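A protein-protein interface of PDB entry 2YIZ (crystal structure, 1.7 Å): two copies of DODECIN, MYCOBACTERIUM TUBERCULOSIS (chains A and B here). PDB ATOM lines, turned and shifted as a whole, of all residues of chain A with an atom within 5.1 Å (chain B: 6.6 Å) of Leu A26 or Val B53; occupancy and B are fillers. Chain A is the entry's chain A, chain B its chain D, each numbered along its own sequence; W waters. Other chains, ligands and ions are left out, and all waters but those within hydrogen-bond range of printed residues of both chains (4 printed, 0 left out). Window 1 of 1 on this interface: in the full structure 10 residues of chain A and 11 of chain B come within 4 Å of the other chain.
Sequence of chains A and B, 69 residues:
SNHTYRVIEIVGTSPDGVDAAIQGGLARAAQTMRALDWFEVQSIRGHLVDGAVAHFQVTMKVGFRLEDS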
ATOM      1  N   ILE A  10      15.165   3.080  -6.259  1.00  0.00           N
ATOM      2  CA  ILE A  10      16.549   2.647  -6.209  1.00  0.00           C
ATOM      3  C   ILE A  10      17.097   2.733  -4.788  1.00  0.00           C
ATOM      4  O   ILE A  10      16.524   3.385  -3.918  1.00  0.00           O
ATOM      5  CB  ILE A  10      17.425   3.488  -7.135  1.00  0.00           C
ATOM      6  CG1 ILE A  10      17.455   4.944  -6.706  1.00  0.00           C
ATOM      7  CG2 ILE A  10      16.983   3.376  -8.614  1.00  0.00           C
ATOM      8  CD1 ILE A  10      18.523   5.758  -7.431  1.00  0.00           C
ATOM      9  N   ALA A  21      25.269   8.398   0.122  1.00  0.00           N
ATOM     10  CA  ALA A  21      24.439   7.311  -0.409  1.00  0.00           C
ATOM     11  C   ALA A  21      23.409   7.819  -1.410  1.00  0.00           C
ATOM     12  O   ALA A  21      23.212   7.231  -2.489  1.00  0.00           O
ATOM     13  CB  ALA A  21      23.769   6.541   0.745  1.00  0.00           C
ATOM     14  N   ILE A  22      22.772   8.940  -1.073  1.00  0.00           N
ATOM     15  CA  ILE A  22      21.828   9.594  -1.968  1.00  0.00           C
ATOM     16  C   ILE A  22      22.514   9.967  -3.264  1.00  0.00           C
ATOM     17  O   ILE A  22      22.065   9.602  -4.356  1.00  0.00           O
ATOM     18  CB  ILE A  22      21.203  10.826  -1.295  1.00  0.00           C
ATOM     19  CG1 ILE A  22      20.219  10.362  -0.206  1.00  0.00           C
ATOM     20  CG2 ILE A  22      20.511  11.718  -2.337  1.00  0.00           C
ATOM     21  CD1 ILE A  22      19.711  11.461   0.696  1.00  0.00           C
ATOM     22  N   GLN A  23      23.636  10.658  -3.131  1.00  0.00           N
ATOM     23  CA  GLN A  23      24.360  11.149  -4.298  1.00  0.00           C
ATOM     24  C   GLN A  23      24.847   9.981  -5.160  1.00  0.00           C
ATOM     25  O   GLN A  23      24.768  10.035  -6.390  1.00  0.00           O
ATOM     26  CB  GLN A  23      25.534  12.019  -3.872  1.00  0.00           C
ATOM     27  CG  GLN A  23      25.164  13.323  -3.169  1.00  0.00           C
ATOM     28  CD  GLN A  23      24.769  14.437  -4.114  1.00  0.00           C
ATOM     29  OE1 GLN A  23      24.427  14.201  -5.286  1.00  0.00           O
ATOM     30  NE2 GLN A  23      24.809  15.671  -3.606  1.00  0.00           N
ATOM     31  N   GLY A  24      25.317   8.913  -4.517  1.00  0.00           N
ATOM     32  CA  GLY A  24      25.816   7.757  -5.257  1.00  0.00           C
ATOM     33  C   GLY A  24      24.740   7.047  -6.058  1.00  0.00           C
ATOM     34  O   GLY A  24      24.947   6.680  -7.233  1.00  0.00           O
ATOM     35  N   GLY A  25      23.592   6.836  -5.423  1.00  0.00           N
ATOM     36  CA  GLY A  25      22.460   6.209  -6.085  1.00  0.00           C
ATOM     37  C   GLY A  25      21.986   7.022  -7.274  1.00  0.00           C
ATOM     38  O   GLY A  25      21.728   6.496  -8.359  1.00  0.00           O
ATOM     39  N   LEU A  26      21.862   8.323  -7.064  1.00  0.00           N
ATOM     40  CA  LEU A  26      21.354   9.198  -8.108  1.00  0.00           C
ATOM     41  C   LEU A  26      22.353   9.288  -9.263  1.00  0.00           C
ATOM     42  O   LEU A  26      21.939   9.346 -10.432  1.00  0.00           O
ATOM     43  CB  LEU A  26      21.007  10.572  -7.538  1.00  0.00           C
ATOM     44  CG  LEU A  26      19.824  10.590  -6.582  1.00  0.00           C
ATOM     45  CD1 LEU A  26      19.698  11.979  -5.927  1.00  0.00           C
ATOM     46  CD2 LEU A  26      18.511  10.162  -7.265  1.00  0.00           C
ATOM     47  N   ALA A  27      23.649   9.267  -8.956  1.00  0.00           N
ATOM     48  CA  ALA A  27      24.686   9.330 -10.003  1.00  0.00           C
ATOM     49  C   ALA A  27      24.605   8.103 -10.897  1.00  0.00           C
ATOM     50  O   ALA A  27      24.757   8.207 -12.127  1.00  0.00           O
ATOM     51  CB  ALA A  27      26.103   9.463  -9.387  1.00  0.00           C
ATOM     52  N   ARG A  28      24.402   6.929 -10.285  1.00  0.00           N
ATOM     53  CA  ARG A  28      24.219   5.705 -11.062  1.00  0.00           C
ATOM     54  C   ARG A  28      22.952   5.796 -11.902  1.00  0.00           C
ATOM     55  O   ARG A  28      22.955   5.436 -13.084  1.00  0.00           O
ATOM     56  CB  ARG A  28      24.157   4.467 -10.149  1.00  0.00           C
ATOM     57  CG  ARG A  28      23.832   3.159 -10.869  1.00  0.00           C
ATOM     58  CD  ARG A  28      24.859   2.836 -11.960  1.00  0.00           C
ATOM     59  NE  ARG A  28      24.471   1.658 -12.738  1.00  0.00           N
ATOM     60  CZ  ARG A  28      23.539   1.639 -13.689  1.00  0.00           C
ATOM     61  NH1 ARG A  28      22.878   2.739 -14.022  1.00  0.00           N
ATOM     62  NH2 ARG A  28      23.266   0.504 -14.320  1.00  0.00           N
ATOM     63  N   ALA A  29      21.869   6.285 -11.312  1.00  0.00           N
ATOM     64  CA  ALA A  29      20.604   6.388 -12.035  1.00  0.00           C
ATOM     65  C   ALA A  29      20.757   7.305 -13.258  1.00  0.00           C
ATOM     66  O   ALA A  29      20.238   7.001 -14.343  1.00  0.00           O
ATOM     67  CB  ALA A  29      19.471   6.880 -11.104  1.00  0.00           C
ATOM     68  N   ALA A  30      21.496   8.400 -13.103  1.00  0.00           N
ATOM     69  CA  ALA A  30      21.612   9.398 -14.174  1.00  0.00           C
ATOM     70  C   ALA A  30      22.352   8.840 -15.386  1.00  0.00           C
ATOM     71  O   ALA A  30      22.095   9.281 -16.517  1.00  0.00           O
ATOM     72  CB  ALA A  30      22.307  10.645 -13.679  1.00  0.00           C
ATOM     73  N   LEU A  36      15.628  13.169 -15.344  1.00  0.00           N
ATOM     74  CA  LEU A  36      15.399  13.039 -13.880  1.00  0.00           C
ATOM     75  C   LEU A  36      14.944  14.378 -13.307  1.00  0.00           C
ATOM     76  O   LEU A  36      15.484  15.433 -13.650  1.00  0.00           O
ATOM     77  CB  LEU A  36      16.660  12.582 -13.153  1.00  0.00           C
ATOM     78  CG  LEU A  36      17.255  11.209 -13.483  1.00  0.00           C
ATOM     79  CD1 LEU A  36      18.379  10.897 -12.482  1.00  0.00           C
ATOM     80  CD2 LEU A  36      16.222  10.085 -13.455  1.00  0.00           C
ATOM     81  N   PHE A  39      13.566  13.360  -6.370  1.00  0.00           N
ATOM     82  CA  PHE A  39      13.628  12.136  -5.571  1.00  0.00           C
ATOM     83  C   PHE A  39      12.970  12.358  -4.221  1.00  0.00           C
ATOM     84  O   PHE A  39      12.766  13.492  -3.774  1.00  0.00           O
ATOM     85  CB  PHE A  39      15.054  11.632  -5.377  1.00  0.00           C
ATOM     86  CG  PHE A  39      15.888  12.469  -4.431  1.00  0.00           C
ATOM     87  CD1 PHE A  39      16.570  13.581  -4.898  1.00  0.00           C
ATOM     88  CD2 PHE A  39      15.977  12.160  -3.087  1.00  0.00           C
ATOM     89  CE1 PHE A  39      17.340  14.346  -4.055  1.00  0.00           C
ATOM     90  CE2 PHE A  39      16.758  12.951  -2.217  1.00  0.00           C
ATOM     91  CZ  PHE A  39      17.421  14.025  -2.707  1.00  0.00           C
ATOM     92  N   MET A  60      15.294   5.401  -2.394  1.00  0.00           N
ATOM     93  CA  MET A  60      14.677   6.584  -2.944  1.00  0.00           C
ATOM     94  C   MET A  60      13.704   6.231  -4.039  1.00  0.00           C
ATOM     95  O   MET A  60      13.985   5.380  -4.875  1.00  0.00           O
ATOM     96  CB  MET A  60      15.733   7.489  -3.597  1.00  0.00           C
ATOM     97  CG  MET A  60      16.777   8.028  -2.601  1.00  0.00           C
ATOM     98  SD  MET A  60      18.185   8.835  -3.381  1.00  0.00           S
ATOM     99  CE  MET A  60      19.188   7.398  -3.769  1.00  0.00           C
ATOM    100  N   VAL A  62      12.460   7.940  -7.474  1.00  0.00           N
ATOM    101  CA  VAL A  62      13.080   8.879  -8.392  1.00  0.00           C
ATOM    102  C   VAL A  62      12.119   9.079  -9.537  1.00  0.00           C
ATOM    103  O   VAL A  62      11.769   8.121 -10.231  1.00  0.00           O
ATOM    104  CB  VAL A  62      14.433   8.374  -8.942  1.00  0.00           C
ATOM    105  CG1 VAL A  62      15.044   9.405  -9.888  1.00  0.00           C
ATOM    106  CG2 VAL A  62      15.382   8.044  -7.782  1.00  0.00           C
ATOM    107  N   SER B  14      18.883  23.180   0.615  1.00  0.00           N
ATOM    108  CA  SER B  14      20.315  23.430   0.395  1.00  0.00           C
ATOM    109  C   SER B  14      20.835  22.462  -0.640  1.00  0.00           C
ATOM    110  O   SER B  14      20.451  21.296  -0.646  1.00  0.00           O
ATOM    111  CB  SER B  14      21.109  23.169   1.670  1.00  0.00           C
ATOM    112  OG  SER B  14      22.509  23.335   1.443  1.00  0.00           O
ATOM    113  N   PRO B  15      21.777  22.907  -1.481  1.00  0.00           N
ATOM    114  CA  PRO B  15      22.431  21.934  -2.341  1.00  0.00           C
ATOM    115  C   PRO B  15      23.398  21.013  -1.601  1.00  0.00           C
ATOM    116  O   PRO B  15      23.775  19.979  -2.156  1.00  0.00           O
ATOM    117  CB  PRO B  15      23.228  22.792  -3.333  1.00  0.00           C
ATOM    118  CG  PRO B  15      23.068  24.167  -2.932  1.00  0.00           C
ATOM    119  CD  PRO B  15      22.250  24.276  -1.708  1.00  0.00           C
ATOM    120  N   ASP B  16      23.739  21.382  -0.361  1.00  0.00           N
ATOM    121  CA  ASP B  16      24.827  20.749   0.402  1.00  0.00           C
ATOM    122  C   ASP B  16      24.406  19.668   1.393  1.00  0.00           C
ATOM    123  O   ASP B  16      25.190  19.315   2.290  1.00  0.00           O
ATOM    124  CB  ASP B  16      25.600  21.823   1.179  1.00  0.00           C
ATOM    125  CG  ASP B  16      26.127  22.929   0.291  1.00  0.00           C
ATOM    126  OD1 ASP B  16      26.320  22.701  -0.925  1.00  0.00           O
ATOM    127  OD2 ASP B  16      26.357  24.035   0.825  1.00  0.00           O
ATOM    128  N   ARG B  45      13.368  15.094   0.309  1.00  0.00           N
ATOM    129  CA  ARG B  45      13.162  15.074  -1.119  1.00  0.00           C
ATOM    130  C   ARG B  45      14.268  15.904  -1.752  1.00  0.00           C
ATOM    131  O   ARG B  45      15.101  16.493  -1.062  1.00  0.00           O
ATOM    132  CB  ARG B  45      11.784  15.661  -1.417  1.00  0.00           C
ATOM    133  CG  ARG B  45      10.662  14.887  -0.758  1.00  0.00           C
ATOM    134  CD  ARG B  45       9.315  15.626  -0.811  1.00  0.00           C
ATOM    135  NE  ARG B  45       8.776  15.536  -2.153  1.00  0.00           N
ATOM    136  CZ  ARG B  45       7.878  14.646  -2.582  1.00  0.00           C
ATOM    137  NH1 ARG B  45       7.330  13.746  -1.761  1.00  0.00           N
ATOM    138  NH2 ARG B  45       7.513  14.669  -3.860  1.00  0.00           N
ATOM    139  N   GLY B  46      14.282  15.975  -3.071  1.00  0.00           N
ATOM    140  CA  GLY B  46      15.152  16.925  -3.739  1.00  0.00           C
ATOM    141  C   GLY B  46      14.776  17.124  -5.178  1.00  0.00           C
ATOM    142  O   GLY B  46      14.077  16.301  -5.776  1.00  0.00           O
ATOM    143  N   HIS B  47      15.267  18.234  -5.725  1.00  0.00           N
ATOM    144  CA  HIS B  47      15.081  18.599  -7.119  1.00  0.00           C
ATOM    145  C   HIS B  47      16.373  18.296  -7.855  1.00  0.00           C
ATOM    146  O   HIS B  47      17.456  18.708  -7.418  1.00  0.00           O
ATOM    147  CB  HIS B  47      14.763  20.091  -7.199  1.00  0.00           C
ATOM    148  CG  HIS B  47      14.537  20.599  -8.587  1.00  0.00           C
ATOM    149  ND1 HIS B  47      13.820  19.892  -9.527  1.00  0.00           N
ATOM    150  CD2 HIS B  47      14.939  21.736  -9.195  1.00  0.00           C
ATOM    151  CE1 HIS B  47      13.791  20.573 -10.657  1.00  0.00           C
ATOM    152  NE2 HIS B  47      14.462  21.696 -10.485  1.00  0.00           N
ATOM    153  N   LEU B  48      16.233  17.601  -8.985  1.00  0.00           N
ATOM    154  CA  LEU B  48      17.334  17.218  -9.843  1.00  0.00           C
ATOM    155  C   LEU B  48      17.379  18.114 -11.093  1.00  0.00           C
ATOM    156  O   LEU B  48      16.347  18.364 -11.713  1.00  0.00           O
ATOM    157  CB  LEU B  48      17.154  15.747 -10.242  1.00  0.00           C
ATOM    158  CG  LEU B  48      17.014  14.825  -9.019  1.00  0.00           C
ATOM    159  CD1 LEU B  48      16.511  13.416  -9.365  1.00  0.00           C
ATOM    160  CD2 LEU B  48      18.383  14.776  -8.351  1.00  0.00           C
ATOM    161  N   VAL B  49      18.568  18.586 -11.438  1.00  0.00           N
ATOM    162  CA  VAL B  49      18.794  19.382 -12.663  1.00  0.00           C
ATOM    163  C   VAL B  49      20.053  18.856 -13.339  1.00  0.00           C
ATOM    164  O   VAL B  49      21.089  18.754 -12.711  1.00  0.00           O
ATOM    165  CB  VAL B  49      18.952  20.885 -12.333  1.00  0.00           C
ATOM    166  CG1 VAL B  49      19.381  21.689 -13.592  1.00  0.00           C
ATOM    167  CG2 VAL B  49      17.659  21.439 -11.714  1.00  0.00           C
ATOM    168  N   GLY B  51      20.845  15.936 -14.055  1.00  0.00           N
ATOM    169  CA  GLY B  51      21.270  14.711 -13.409  1.00  0.00           C
ATOM    170  C   GLY B  51      21.904  14.867 -12.043  1.00  0.00           C
ATOM    171  O   GLY B  51      22.270  13.856 -11.447  1.00  0.00           O
ATOM    172  N   ALA B  52      22.005  16.100 -11.536  1.00  0.00           N
ATOM    173  CA  ALA B  52      22.629  16.413 -10.244  1.00  0.00           C
ATOM    174  C   ALA B  52      21.596  16.938  -9.256  1.00  0.00           C
ATOM    175  O   ALA B  52      20.552  17.413  -9.663  1.00  0.00           O
ATOM    176  CB  ALA B  52      23.729  17.463 -10.457  1.00  0.00           C
ATOM    177  N   VAL B  53      21.848  16.816  -7.948  1.00  0.00           N
ATOM    178  CA  VAL B  53      20.938  17.393  -6.956  1.00  0.00           C
ATOM    179  C   VAL B  53      21.144  18.902  -6.859  1.00  0.00           C
ATOM    180  O   VAL B  53      22.207  19.379  -6.415  1.00  0.00           O
ATOM    181  CB  VAL B  53      21.111  16.758  -5.557  1.00  0.00           C
ATOM    182  CG1 VAL B  53      20.093  17.381  -4.579  1.00  0.00           C
ATOM    183  CG2 VAL B  53      20.979  15.241  -5.662  1.00  0.00           C
ATOM    184  N   ALA B  54      20.149  19.661  -7.324  1.00  0.00           N
ATOM    185  CA  ALA B  54      20.177  21.106  -7.226  1.00  0.00           C
ATOM    186  C   ALA B  54      19.870  21.588  -5.811  1.00  0.00           C
ATOM    187  O   ALA B  54      20.514  22.502  -5.312  1.00  0.00           O
ATOM    188  CB  ALA B  54      19.198  21.719  -8.232  1.00  0.00           C
ATOM    189  N   HIS B  55      18.851  21.000  -5.184  1.00  0.00           N
ATOM    190  CA  HIS B  55      18.545  21.240  -3.770  1.00  0.00           C
ATOM    191  C   HIS B  55      17.999  20.006  -3.110  1.00  0.00           C
ATOM    192  O   HIS B  55      17.077  19.371  -3.658  1.00  0.00           O
ATOM    193  CB  HIS B  55      17.490  22.323  -3.598  1.00  0.00           C
ATOM    194  CG  HIS B  55      17.992  23.701  -3.867  1.00  0.00           C
ATOM    195  ND1 HIS B  55      17.918  24.269  -5.114  1.00  0.00           N
ATOM    196  CD2 HIS B  55      18.582  24.620  -3.062  1.00  0.00           C
ATOM    197  CE1 HIS B  55      18.443  25.484  -5.073  1.00  0.00           C
ATOM    198  NE2 HIS B  55      18.855  25.719  -3.839  1.00  0.00           N
ATOM    199  N   PHE B  56      18.542  19.692  -1.931  1.00  0.00           N
ATOM    200  CA  PHE B  56      17.890  18.836  -0.944  1.00  0.00           C
ATOM    201  C   PHE B  56      16.781  19.671  -0.312  1.00  0.00           C
ATOM    202  O   PHE B  56      16.967  20.880  -0.050  1.00  0.00           O
ATOM    203  CB  PHE B  56      18.849  18.363   0.174  1.00  0.00           C
ATOM    204  CG  PHE B  56      19.951  17.434  -0.306  1.00  0.00           C
ATOM    205  CD1 PHE B  56      21.025  17.904  -1.056  1.00  0.00           C
ATOM    206  CD2 PHE B  56      19.896  16.090   0.000  1.00  0.00           C
ATOM    207  CE1 PHE B  56      22.024  17.037  -1.485  1.00  0.00           C
ATOM    208  CE2 PHE B  56      20.897  15.212  -0.423  1.00  0.00           C
ATOM    209  CZ  PHE B  56      21.949  15.687  -1.175  1.00  0.00           C
ATOM    210  N   GLN B  57      15.644  19.030  -0.059  1.00  0.00           N
ATOM    211  CA  GLN B  57      14.450  19.692   0.477  1.00  0.00           C
ATOM    212  C   GLN B  57      13.963  18.854   1.659  1.00  0.00           C
ATOM    213  O   GLN B  57      13.519  17.722   1.478  1.00  0.00           O
ATOM    214  CB  GLN B  57      13.368  19.787  -0.574  1.00  0.00           C
ATOM    215  CG  GLN B  57      13.771  20.572  -1.793  1.00  0.00           C
ATOM    216  CD  GLN B  57      12.950  20.252  -3.007  1.00  0.00           C
ATOM    217  OE1 GLN B  57      12.415  19.162  -3.133  1.00  0.00           O
ATOM    218  NE2 GLN B  57      12.855  21.213  -3.931  1.00  0.00           N
HETATM  219  O   HOH W   1      24.487  16.069  -7.268  1.00  0.00           O
HETATM  220  O   HOH W   2      18.016  16.029 -14.340  1.00  0.00           O
HETATM  221  O   HOH W   3      14.851  18.674 -13.876  1.00  0.00           O
HETATM  222  O   HOH W   4      24.109  18.556  -4.547  1.00  0.00           O
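The backbone carbonyl oxygen (O) of Phe A39 sits at hydrogen-bond distance from the backbone NH (N) of Gly B46, 3.0 Å away.
No position is printed for both chains.
Water W3 bridges the backbone carbonyl oxygen of Leu B48 (2.6 Å) and the backbone carbonyl oxygen of Leu A36 (3.3 Å). Water W2 lies within hydrogen-bond range of the backbone carbonyl oxygen (O) of Leu A36 and the backbone NH (N) of Gly B51. Water W1 bridges the side-chain amide oxygen of Gln A23 and the backbone NH of Val B53. Water W4 lies within hydrogen-bond range of the backbone carbonyl oxygen of Val B53 (2.8 Å), the backbone carbonyl oxygen of Pro B15 (2.8 Å) and the side-chain amide nitrogen of Gln A23 (3.1 Å).
Gln A23 touches Val B53 (OE1 to CG2, 3.6 Å). Gln A23 touches Phe B56. Leu A26 touches Leu B48. CD1 of Leu A26 touches CG2 of Val B53, at 3.5 Å. Ala A30 touches Gly B51 (CB to O, 3.9 Å). O of Leu A36 touches O of Leu B48, at 3.6 Å. Phe A39 touches Arg B45 (O to CA, 3.1 Å).
Hydrophobic or aromatic side chains of chain B that line the printed part of chain A: Leu B48, Val B53 and Phe B56. Among the printed residues, 8 pairs touch across the chains.
The backbone NH (N) of Phe B56 is in hydrogen-bond range of the backbone carbonyl oxygen (O) of Ser B14, at 2.8 Å. The backbone NH (N) of Gln B57 is in hydrogen-bond range of the backbone carbonyl oxygen (O) of Arg B45, 2.8 Å away.
Of the printed residues of chain A, Gly B46 touches Phe A39 (3.0 Å). Printed residues of chain A within 4 Å of Phe B56: Gln A23. Printed residues of chain A within 4 Å of Arg B45: Phe A39 (3.1 Å). Printed residues of chain B within 4 Å of Phe A39: Arg B45 (3.1 Å) and Gly B46 (3.0 Å). Gly A25 touches none of the printed residues of chain B. Val B49 touches none of the printed residues of chain A. The nearest printed residue of chain B that does not touch Leu A26 is Gly B51 (4.6 Å).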
